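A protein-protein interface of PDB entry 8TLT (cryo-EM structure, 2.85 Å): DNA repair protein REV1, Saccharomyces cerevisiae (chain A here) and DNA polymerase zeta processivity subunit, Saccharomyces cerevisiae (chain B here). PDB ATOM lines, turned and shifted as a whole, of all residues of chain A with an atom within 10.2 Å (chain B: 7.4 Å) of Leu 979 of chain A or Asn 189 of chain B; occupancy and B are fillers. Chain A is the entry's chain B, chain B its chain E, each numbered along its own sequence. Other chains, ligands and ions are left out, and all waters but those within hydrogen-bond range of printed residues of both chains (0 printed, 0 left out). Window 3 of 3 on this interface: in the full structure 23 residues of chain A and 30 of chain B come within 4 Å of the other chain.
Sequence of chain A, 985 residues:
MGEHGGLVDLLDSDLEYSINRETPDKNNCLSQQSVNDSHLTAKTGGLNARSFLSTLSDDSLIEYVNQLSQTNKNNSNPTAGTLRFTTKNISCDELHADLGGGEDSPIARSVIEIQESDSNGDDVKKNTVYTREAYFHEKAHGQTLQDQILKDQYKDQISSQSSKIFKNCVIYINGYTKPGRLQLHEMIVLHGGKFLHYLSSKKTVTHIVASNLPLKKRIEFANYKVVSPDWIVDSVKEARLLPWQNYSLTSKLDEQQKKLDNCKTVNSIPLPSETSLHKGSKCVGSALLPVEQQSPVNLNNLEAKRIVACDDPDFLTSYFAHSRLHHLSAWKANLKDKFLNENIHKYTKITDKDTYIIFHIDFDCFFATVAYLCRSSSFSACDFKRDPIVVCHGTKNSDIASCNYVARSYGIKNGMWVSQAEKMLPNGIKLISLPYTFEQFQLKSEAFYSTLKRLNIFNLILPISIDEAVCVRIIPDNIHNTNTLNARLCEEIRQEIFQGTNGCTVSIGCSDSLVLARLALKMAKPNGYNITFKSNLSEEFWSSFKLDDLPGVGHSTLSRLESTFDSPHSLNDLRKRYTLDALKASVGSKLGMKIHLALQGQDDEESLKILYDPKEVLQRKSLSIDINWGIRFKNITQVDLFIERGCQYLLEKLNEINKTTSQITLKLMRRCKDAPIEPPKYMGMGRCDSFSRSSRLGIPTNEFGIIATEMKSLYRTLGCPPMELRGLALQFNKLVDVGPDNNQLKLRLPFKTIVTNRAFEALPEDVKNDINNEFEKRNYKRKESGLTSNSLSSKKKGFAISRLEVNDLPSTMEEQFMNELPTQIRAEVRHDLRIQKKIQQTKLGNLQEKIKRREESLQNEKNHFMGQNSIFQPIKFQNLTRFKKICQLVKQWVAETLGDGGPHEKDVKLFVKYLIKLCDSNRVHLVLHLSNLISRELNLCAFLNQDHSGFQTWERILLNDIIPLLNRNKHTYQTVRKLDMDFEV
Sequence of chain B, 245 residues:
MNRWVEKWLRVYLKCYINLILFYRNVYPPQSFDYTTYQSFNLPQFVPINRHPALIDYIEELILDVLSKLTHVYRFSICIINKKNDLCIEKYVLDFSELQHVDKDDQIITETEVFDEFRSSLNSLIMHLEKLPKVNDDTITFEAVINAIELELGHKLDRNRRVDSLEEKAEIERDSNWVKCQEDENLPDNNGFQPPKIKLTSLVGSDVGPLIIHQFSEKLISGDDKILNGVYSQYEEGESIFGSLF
The backbone carbonyl oxygen (O) of Lys 196 of chain B lies close to the backbone carbonyl oxygen (O) of Leu 219 of chain B (2.7 Å).
Among the printed residues, merely in contact across the chains: Leu 979 of chain A with Asn 189 of chain B (3.3 Å), Leu 979 of chain A with Pro 195 of chain B (3.5 Å), Lys 978 of chain A with Pro 187 of chain B (3.5 Å), Met 981 of chain A with Ile 197 of chain B (3.6 Å), Leu 979 of chain A with Leu 186 of chain B (3.6 Å), Asp 980 of chain A with Lys 196 of chain B (3.6 Å) and Leu 979 of chain A with Pro 187 of chain B (3.7 Å).
Leu 979 of chain A touches just these residues of chain B: Leu 186, Pro 187, Asn 189 and Pro 195.
Of the printed residues of chain B, Met 981 of chain A touches Ile 197 (3.6 Å).
Printed residues of chain B within 4 Å of Asp 982 of chain A: Ile 197.
Printed residues of chain A within 4 Å of Asp 183 of chain B: Lys 978.
Pro 187 of chain B touches two residues of chain A.
No residue of chain A comes within 4 Å of Asp 188 of chain B.
Asn 189 of chain B touches one residue of chain A.
Pro 194 of chain B touches none of the printed residues of chain A.
Pro 195 of chain B touches just one residue of chain A: Leu 979.
Of the printed residues of chain A, Ile 197 of chain B touches Asp 980 (3.1 Å), Met 981 (3.6 Å) and Asp 982 (2.9 Å).
The backbone carbonyl oxygen of Asp 183 of chain B is in hydrogen-bond range of the side-chain amino group of Lys 978 of chain A (2.4 Å).
NZ of Lys 978 of chain A sits at hydrogen-bond distance from O of Leu 186 of chain B.
O of Asp 980 of chain A sits at hydrogen-bond distance from N of Ile 197 of chain B (3.1 Å).
O of Ile 197 of chain B lies within hydrogen-bond range of N of Asp 982 of chain A (2.9 Å).
Of the 14 printed residues of chain B, 7 touch a printed residue of chain A.
Printed residues of chain B that touch a printed residue of chain A: Asp 183, Leu 186, Pro 187, Asn 189, Pro 195, Lys 196 and Ile 197.
Hydrophobic or aromatic side chains of chain B within 4 Å of the printed part of chain A: Leu 186 and Ile 197.
Hydrophobic or aromatic side chains of chain A within 4 Å of the printed part of chain B: Leu 979 and Met 981.
Among the printed residues, no Asp or Glu carboxylate lies within 4 Å of a Lys or Arg side-chain nitrogen of the other chain.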
ATOM      1  N   ASN A 967      17.996  26.690  40.327  1.00  0.00           N
ATOM      2  CA  ASN A 967      17.715  27.799  39.425  1.00  0.00           C
ATOM      3  C   ASN A 967      18.576  29.024  39.706  1.00  0.00           C
ATOM      4  O   ASN A 967      18.128  30.157  39.487  1.00  0.00           O
ATOM      5  CB  ASN A 967      16.232  28.166  39.495  1.00  0.00           C
ATOM      6  CG  ASN A 967      15.335  27.072  38.949  1.00  0.00           C
ATOM      7  N   LYS A 970      23.421  30.781  36.720  1.00  0.00           N
ATOM      8  CA  LYS A 970      23.334  30.325  35.332  1.00  0.00           C
ATOM      9  C   LYS A 970      24.454  30.967  34.509  1.00  0.00           C
ATOM     10  O   LYS A 970      24.238  31.810  33.638  1.00  0.00           O
ATOM     11  CB  LYS A 970      21.962  30.644  34.753  1.00  0.00           C
ATOM     12  CG  LYS A 970      21.010  31.305  35.737  1.00  0.00           C
ATOM     13  N   HIS A 971      25.680  30.538  34.806  1.00  0.00           N
ATOM     14  CA  HIS A 971      26.868  31.036  34.133  1.00  0.00           C
ATOM     15  C   HIS A 971      27.693  29.868  33.612  1.00  0.00           C
ATOM     16  O   HIS A 971      27.750  28.802  34.232  1.00  0.00           O
ATOM     17  CB  HIS A 971      27.722  31.904  35.068  1.00  0.00           C
ATOM     18  N   THR A 972      28.331  30.079  32.463  1.00  0.00           N
ATOM     19  CA  THR A 972      29.157  29.074  31.799  1.00  0.00           C
ATOM     20  C   THR A 972      30.532  29.647  31.477  1.00  0.00           C
ATOM     21  O   THR A 972      31.036  29.529  30.358  1.00  0.00           O
ATOM     22  CB  THR A 972      28.490  28.558  30.525  1.00  0.00           C
ATOM     23  OG1 THR A 972      28.436  29.609  29.553  1.00  0.00           O
ATOM     24  CG2 THR A 972      27.079  28.063  30.813  1.00  0.00           C
ATOM     25  N   VAL A 976      26.040  34.666  30.483  1.00  0.00           N
ATOM     26  CA  VAL A 976      25.018  33.762  30.990  1.00  0.00           C
ATOM     27  C   VAL A 976      24.471  32.934  29.837  1.00  0.00           C
ATOM     28  O   VAL A 976      24.526  33.329  28.672  1.00  0.00           O
ATOM     29  CB  VAL A 976      23.874  34.515  31.705  1.00  0.00           C
ATOM     30  CG1 VAL A 976      24.363  35.095  33.021  1.00  0.00           C
ATOM     31  CG2 VAL A 976      23.321  35.609  30.807  1.00  0.00           C
ATOM     32  N   ARG A 977      23.938  31.765  30.184  1.00  0.00           N
ATOM     33  CA  ARG A 977      23.391  30.860  29.183  1.00  0.00           C
ATOM     34  C   ARG A 977      22.081  31.398  28.623  1.00  0.00           C
ATOM     35  O   ARG A 977      21.290  32.022  29.336  1.00  0.00           O
ATOM     36  CB  ARG A 977      23.176  29.473  29.789  1.00  0.00           C
ATOM     37  CG  ARG A 977      22.732  28.417  28.795  1.00  0.00           C
ATOM     38  CD  ARG A 977      23.597  27.175  28.880  1.00  0.00           C
ATOM     39  NE  ARG A 977      23.373  26.283  27.749  1.00  0.00           N
ATOM     40  CZ  ARG A 977      23.477  24.964  27.804  1.00  0.00           C
ATOM     41  NH1 ARG A 977      23.804  24.343  28.925  1.00  0.00           N
ATOM     42  NH2 ARG A 977      23.249  24.248  26.706  1.00  0.00           N
ATOM     43  N   LYS A 978      21.855  31.157  27.333  1.00  0.00           N
ATOM     44  CA  LYS A 978      20.614  31.563  26.694  1.00  0.00           C
ATOM     45  C   LYS A 978      19.468  30.650  27.126  1.00  0.00           C
ATOM     46  O   LYS A 978      19.674  29.541  27.628  1.00  0.00           O
ATOM     47  CB  LYS A 978      20.766  31.542  25.172  1.00  0.00           C
ATOM     48  CG  LYS A 978      19.751  32.398  24.428  1.00  0.00           C
ATOM     49  CD  LYS A 978      20.070  32.502  22.944  1.00  0.00           C
ATOM     50  CE  LYS A 978      20.659  31.211  22.400  1.00  0.00           C
ATOM     51  NZ  LYS A 978      21.430  31.444  21.149  1.00  0.00           N
ATOM     52  N   LEU A 979      18.242  31.143  26.932  1.00  0.00           N
ATOM     53  CA  LEU A 979      17.019  30.430  27.289  1.00  0.00           C
ATOM     54  C   LEU A 979      16.969  30.123  28.780  1.00  0.00           C
ATOM     55  O   LEU A 979      17.751  30.674  29.562  1.00  0.00           O
ATOM     56  CB  LEU A 979      16.875  29.141  26.474  1.00  0.00           C
ATOM     57  CG  LEU A 979      17.062  29.254  24.959  1.00  0.00           C
ATOM     58  CD1 LEU A 979      17.192  27.879  24.332  1.00  0.00           C
ATOM     59  CD2 LEU A 979      15.914  30.022  24.330  1.00  0.00           C
ATOM     60  N   ASP A 980      16.048  29.254  29.185  1.00  0.00           N
ATOM     61  CA  ASP A 980      15.833  28.941  30.587  1.00  0.00           C
ATOM     62  C   ASP A 980      16.112  27.466  30.849  1.00  0.00           C
ATOM     63  O   ASP A 980      16.107  26.634  29.938  1.00  0.00           O
ATOM     64  CB  ASP A 980      14.405  29.293  31.021  1.00  0.00           C
ATOM     65  CG  ASP A 980      14.339  30.591  31.803  1.00  0.00           C
ATOM     66  OD1 ASP A 980      15.170  31.485  31.543  1.00  0.00           O
ATOM     67  OD2 ASP A 980      13.453  30.719  32.675  1.00  0.00           O
ATOM     68  N   MET A 981      16.349  27.158  32.121  1.00  0.00           N
ATOM     69  CA  MET A 981      16.707  25.814  32.551  1.00  0.00           C
ATOM     70  C   MET A 981      15.451  25.020  32.885  1.00  0.00           C
ATOM     71  O   MET A 981      14.574  25.505  33.607  1.00  0.00           O
ATOM     72  CB  MET A 981      17.627  25.881  33.772  1.00  0.00           C
ATOM     73  CG  MET A 981      19.106  26.133  33.477  1.00  0.00           C
ATOM     74  SD  MET A 981      19.647  25.817  31.785  1.00  0.00           S
ATOM     75  CE  MET A 981      19.615  24.024  31.743  1.00  0.00           C
ATOM     76  N   ASP A 982      15.365  23.801  32.353  1.00  0.00           N
ATOM     77  CA  ASP A 982      14.279  22.867  32.654  1.00  0.00           C
ATOM     78  C   ASP A 982      14.932  21.554  33.076  1.00  0.00           C
ATOM     79  O   ASP A 982      15.165  20.670  32.249  1.00  0.00           O
ATOM     80  CB  ASP A 982      13.351  22.687  31.459  1.00  0.00           C
ATOM     81  CG  ASP A 982      12.232  21.702  31.732  1.00  0.00           C
ATOM     82  N   PHE A 983      15.224  21.428  34.365  1.00  0.00           N
ATOM     83  CA  PHE A 983      15.980  20.294  34.867  1.00  0.00           C
ATOM     84  C   PHE A 983      15.114  19.043  34.956  1.00  0.00           C
ATOM     85  O   PHE A 983      13.897  19.113  35.147  1.00  0.00           O
ATOM     86  CB  PHE A 983      16.572  20.623  36.235  1.00  0.00           C
ATOM     87  CG  PHE A 983      17.562  21.746  36.201  1.00  0.00           C
ATOM     88  CD1 PHE A 983      18.604  21.735  35.292  1.00  0.00           C
ATOM     89  CD2 PHE A 983      17.434  22.824  37.055  1.00  0.00           C
ATOM     90  CE1 PHE A 983      19.513  22.769  35.250  1.00  0.00           C
ATOM     91  CE2 PHE A 983      18.338  23.862  37.014  1.00  0.00           C
ATOM     92  CZ  PHE A 983      19.380  23.834  36.113  1.00  0.00           C
ATOM     93  N   ASP B 183      25.982  28.537  22.743  1.00  0.00           N
ATOM     94  CA  ASP B 183      24.564  28.499  22.378  1.00  0.00           C
ATOM     95  C   ASP B 183      24.309  29.240  21.068  1.00  0.00           C
ATOM     96  O   ASP B 183      23.333  29.978  20.924  1.00  0.00           O
ATOM     97  CB  ASP B 183      23.693  29.062  23.504  1.00  0.00           C
ATOM     98  N   LEU B 186      21.211  27.638  19.129  1.00  0.00           N
ATOM     99  CA  LEU B 186      19.935  27.605  19.823  1.00  0.00           C
ATOM    100  C   LEU B 186      19.013  28.714  19.318  1.00  0.00           C
ATOM    101  O   LEU B 186      19.480  29.734  18.803  1.00  0.00           O
ATOM    102  CB  LEU B 186      20.150  27.753  21.326  1.00  0.00           C
ATOM    103  CG  LEU B 186      20.823  26.574  22.035  1.00  0.00           C
ATOM    104  CD1 LEU B 186      20.441  26.539  23.503  1.00  0.00           C
ATOM    105  CD2 LEU B 186      20.467  25.257  21.361  1.00  0.00           C
ATOM    106  N   PRO B 187      17.697  28.532  19.443  1.00  0.00           N
ATOM    107  CA  PRO B 187      16.768  29.602  19.065  1.00  0.00           C
ATOM    108  C   PRO B 187      16.987  30.850  19.908  1.00  0.00           C
ATOM    109  O   PRO B 187      17.434  30.785  21.054  1.00  0.00           O
ATOM    110  CB  PRO B 187      15.385  28.987  19.319  1.00  0.00           C
ATOM    111  CG  PRO B 187      15.633  27.774  20.157  1.00  0.00           C
ATOM    112  CD  PRO B 187      16.992  27.287  19.783  1.00  0.00           C
ATOM    113  N   ASP B 188      16.664  32.001  19.319  1.00  0.00           N
ATOM    114  CA  ASP B 188      17.045  33.299  19.859  1.00  0.00           C
ATOM    115  C   ASP B 188      16.051  33.846  20.881  1.00  0.00           C
ATOM    116  O   ASP B 188      15.988  35.067  21.066  1.00  0.00           O
ATOM    117  CB  ASP B 188      17.226  34.307  18.721  1.00  0.00           C
ATOM    118  N   ASN B 189      15.280  32.980  21.543  1.00  0.00           N
ATOM    119  CA  ASN B 189      14.357  33.382  22.606  1.00  0.00           C
ATOM    120  C   ASN B 189      13.334  34.398  22.084  1.00  0.00           C
ATOM    121  O   ASN B 189      13.303  35.566  22.480  1.00  0.00           O
ATOM    122  CB  ASN B 189      15.125  33.939  23.812  1.00  0.00           C
ATOM    123  CG  ASN B 189      14.547  33.482  25.135  1.00  0.00           C
ATOM    124  OD1 ASN B 189      13.864  32.462  25.206  1.00  0.00           O
ATOM    125  ND2 ASN B 189      14.819  34.237  26.192  1.00  0.00           N
ATOM    126  N   ASN B 190      12.497  33.908  21.164  1.00  0.00           N
ATOM    127  CA  ASN B 190      11.528  34.770  20.492  1.00  0.00           C
ATOM    128  C   ASN B 190      10.587  35.454  21.477  1.00  0.00           C
ATOM    129  O   ASN B 190      10.158  36.588  21.236  1.00  0.00           O
ATOM    130  CB  ASN B 190      10.726  33.959  19.473  1.00  0.00           C
ATOM    131  N   GLY B 191      10.254  34.791  22.582  1.00  0.00           N
ATOM    132  CA  GLY B 191       9.392  35.351  23.598  1.00  0.00           C
ATOM    133  C   GLY B 191       7.959  34.863  23.554  1.00  0.00           C
ATOM    134  O   GLY B 191       7.244  34.996  24.554  1.00  0.00           O
ATOM    135  N   PHE B 192       7.519  34.304  22.429  1.00  0.00           N
ATOM    136  CA  PHE B 192       6.185  33.719  22.316  1.00  0.00           C
ATOM    137  C   PHE B 192       6.298  32.246  22.682  1.00  0.00           C
ATOM    138  O   PHE B 192       6.621  31.409  21.835  1.00  0.00           O
ATOM    139  CB  PHE B 192       5.623  33.913  20.913  1.00  0.00           C
ATOM    140  N   GLN B 193       6.019  31.929  23.951  1.00  0.00           N
ATOM    141  CA  GLN B 193       6.255  30.605  24.521  1.00  0.00           C
ATOM    142  C   GLN B 193       7.697  30.192  24.252  1.00  0.00           C
ATOM    143  O   GLN B 193       7.945  29.285  23.448  1.00  0.00           O
ATOM    144  CB  GLN B 193       5.277  29.576  23.948  1.00  0.00           C
ATOM    145  N   PRO B 194       8.667  30.840  24.893  1.00  0.00           N
ATOM    146  CA  PRO B 194      10.077  30.595  24.568  1.00  0.00           C
ATOM    147  C   PRO B 194      10.474  29.163  24.868  1.00  0.00           C
ATOM    148  O   PRO B 194       9.999  28.568  25.847  1.00  0.00           O
ATOM    149  CB  PRO B 194      10.829  31.581  25.477  1.00  0.00           C
ATOM    150  CG  PRO B 194       9.797  32.562  25.941  1.00  0.00           C
ATOM    151  CD  PRO B 194       8.517  31.802  25.996  1.00  0.00           C
ATOM    152  N   PRO B 195      11.336  28.571  24.043  1.00  0.00           N
ATOM    153  CA  PRO B 195      11.848  27.232  24.350  1.00  0.00           C
ATOM    154  C   PRO B 195      12.708  27.242  25.604  1.00  0.00           C
ATOM    155  O   PRO B 195      13.404  28.215  25.903  1.00  0.00           O
ATOM    156  CB  PRO B 195      12.676  26.872  23.111  1.00  0.00           C
ATOM    157  CG  PRO B 195      12.234  27.825  22.046  1.00  0.00           C
ATOM    158  CD  PRO B 195      11.841  29.077  22.758  1.00  0.00           C
ATOM    159  N   LYS B 196      12.650  26.137  26.342  1.00  0.00           N
ATOM    160  CA  LYS B 196      13.436  25.953  27.555  1.00  0.00           C
ATOM    161  C   LYS B 196      14.301  24.714  27.387  1.00  0.00           C
ATOM    162  O   LYS B 196      13.778  23.611  27.211  1.00  0.00           O
ATOM    163  CB  LYS B 196      12.535  25.813  28.783  1.00  0.00           C
ATOM    164  CG  LYS B 196      11.222  26.567  28.686  1.00  0.00           C
ATOM    165  CD  LYS B 196      10.650  26.856  30.063  1.00  0.00           C
ATOM    166  N   ILE B 197      15.621  24.895  27.455  1.00  0.00           N
ATOM    167  CA  ILE B 197      16.538  23.773  27.308  1.00  0.00           C
ATOM    168  C   ILE B 197      16.396  22.834  28.502  1.00  0.00           C
ATOM    169  O   ILE B 197      16.227  23.272  29.648  1.00  0.00           O
ATOM    170  CB  ILE B 197      17.980  24.288  27.135  1.00  0.00           C
ATOM    171  CG1 ILE B 197      18.877  23.212  26.521  1.00  0.00           C
ATOM    172  CG2 ILE B 197      18.552  24.814  28.442  1.00  0.00           C
ATOM    173  CD1 ILE B 197      18.408  22.737  25.172  1.00  0.00           C
ATOM    174  N   LEU B 219      16.032  20.411  23.631  1.00  0.00           N
ATOM    175  CA  LEU B 219      15.103  21.538  23.601  1.00  0.00           C
ATOM    176  C   LEU B 219      13.792  21.191  24.297  1.00  0.00           C
ATOM    177  O   LEU B 219      13.336  21.925  25.182  1.00  0.00           O
ATOM    178  CB  LEU B 219      14.846  21.973  22.157  1.00  0.00           C
ATOM    179  CG  LEU B 219      15.967  22.732  21.448  1.00  0.00           C
ATOM    180  CD1 LEU B 219      15.518  23.171  20.067  1.00  0.00           C
ATOM    181  CD2 LEU B 219      16.395  23.930  22.274  1.00  0.00           C
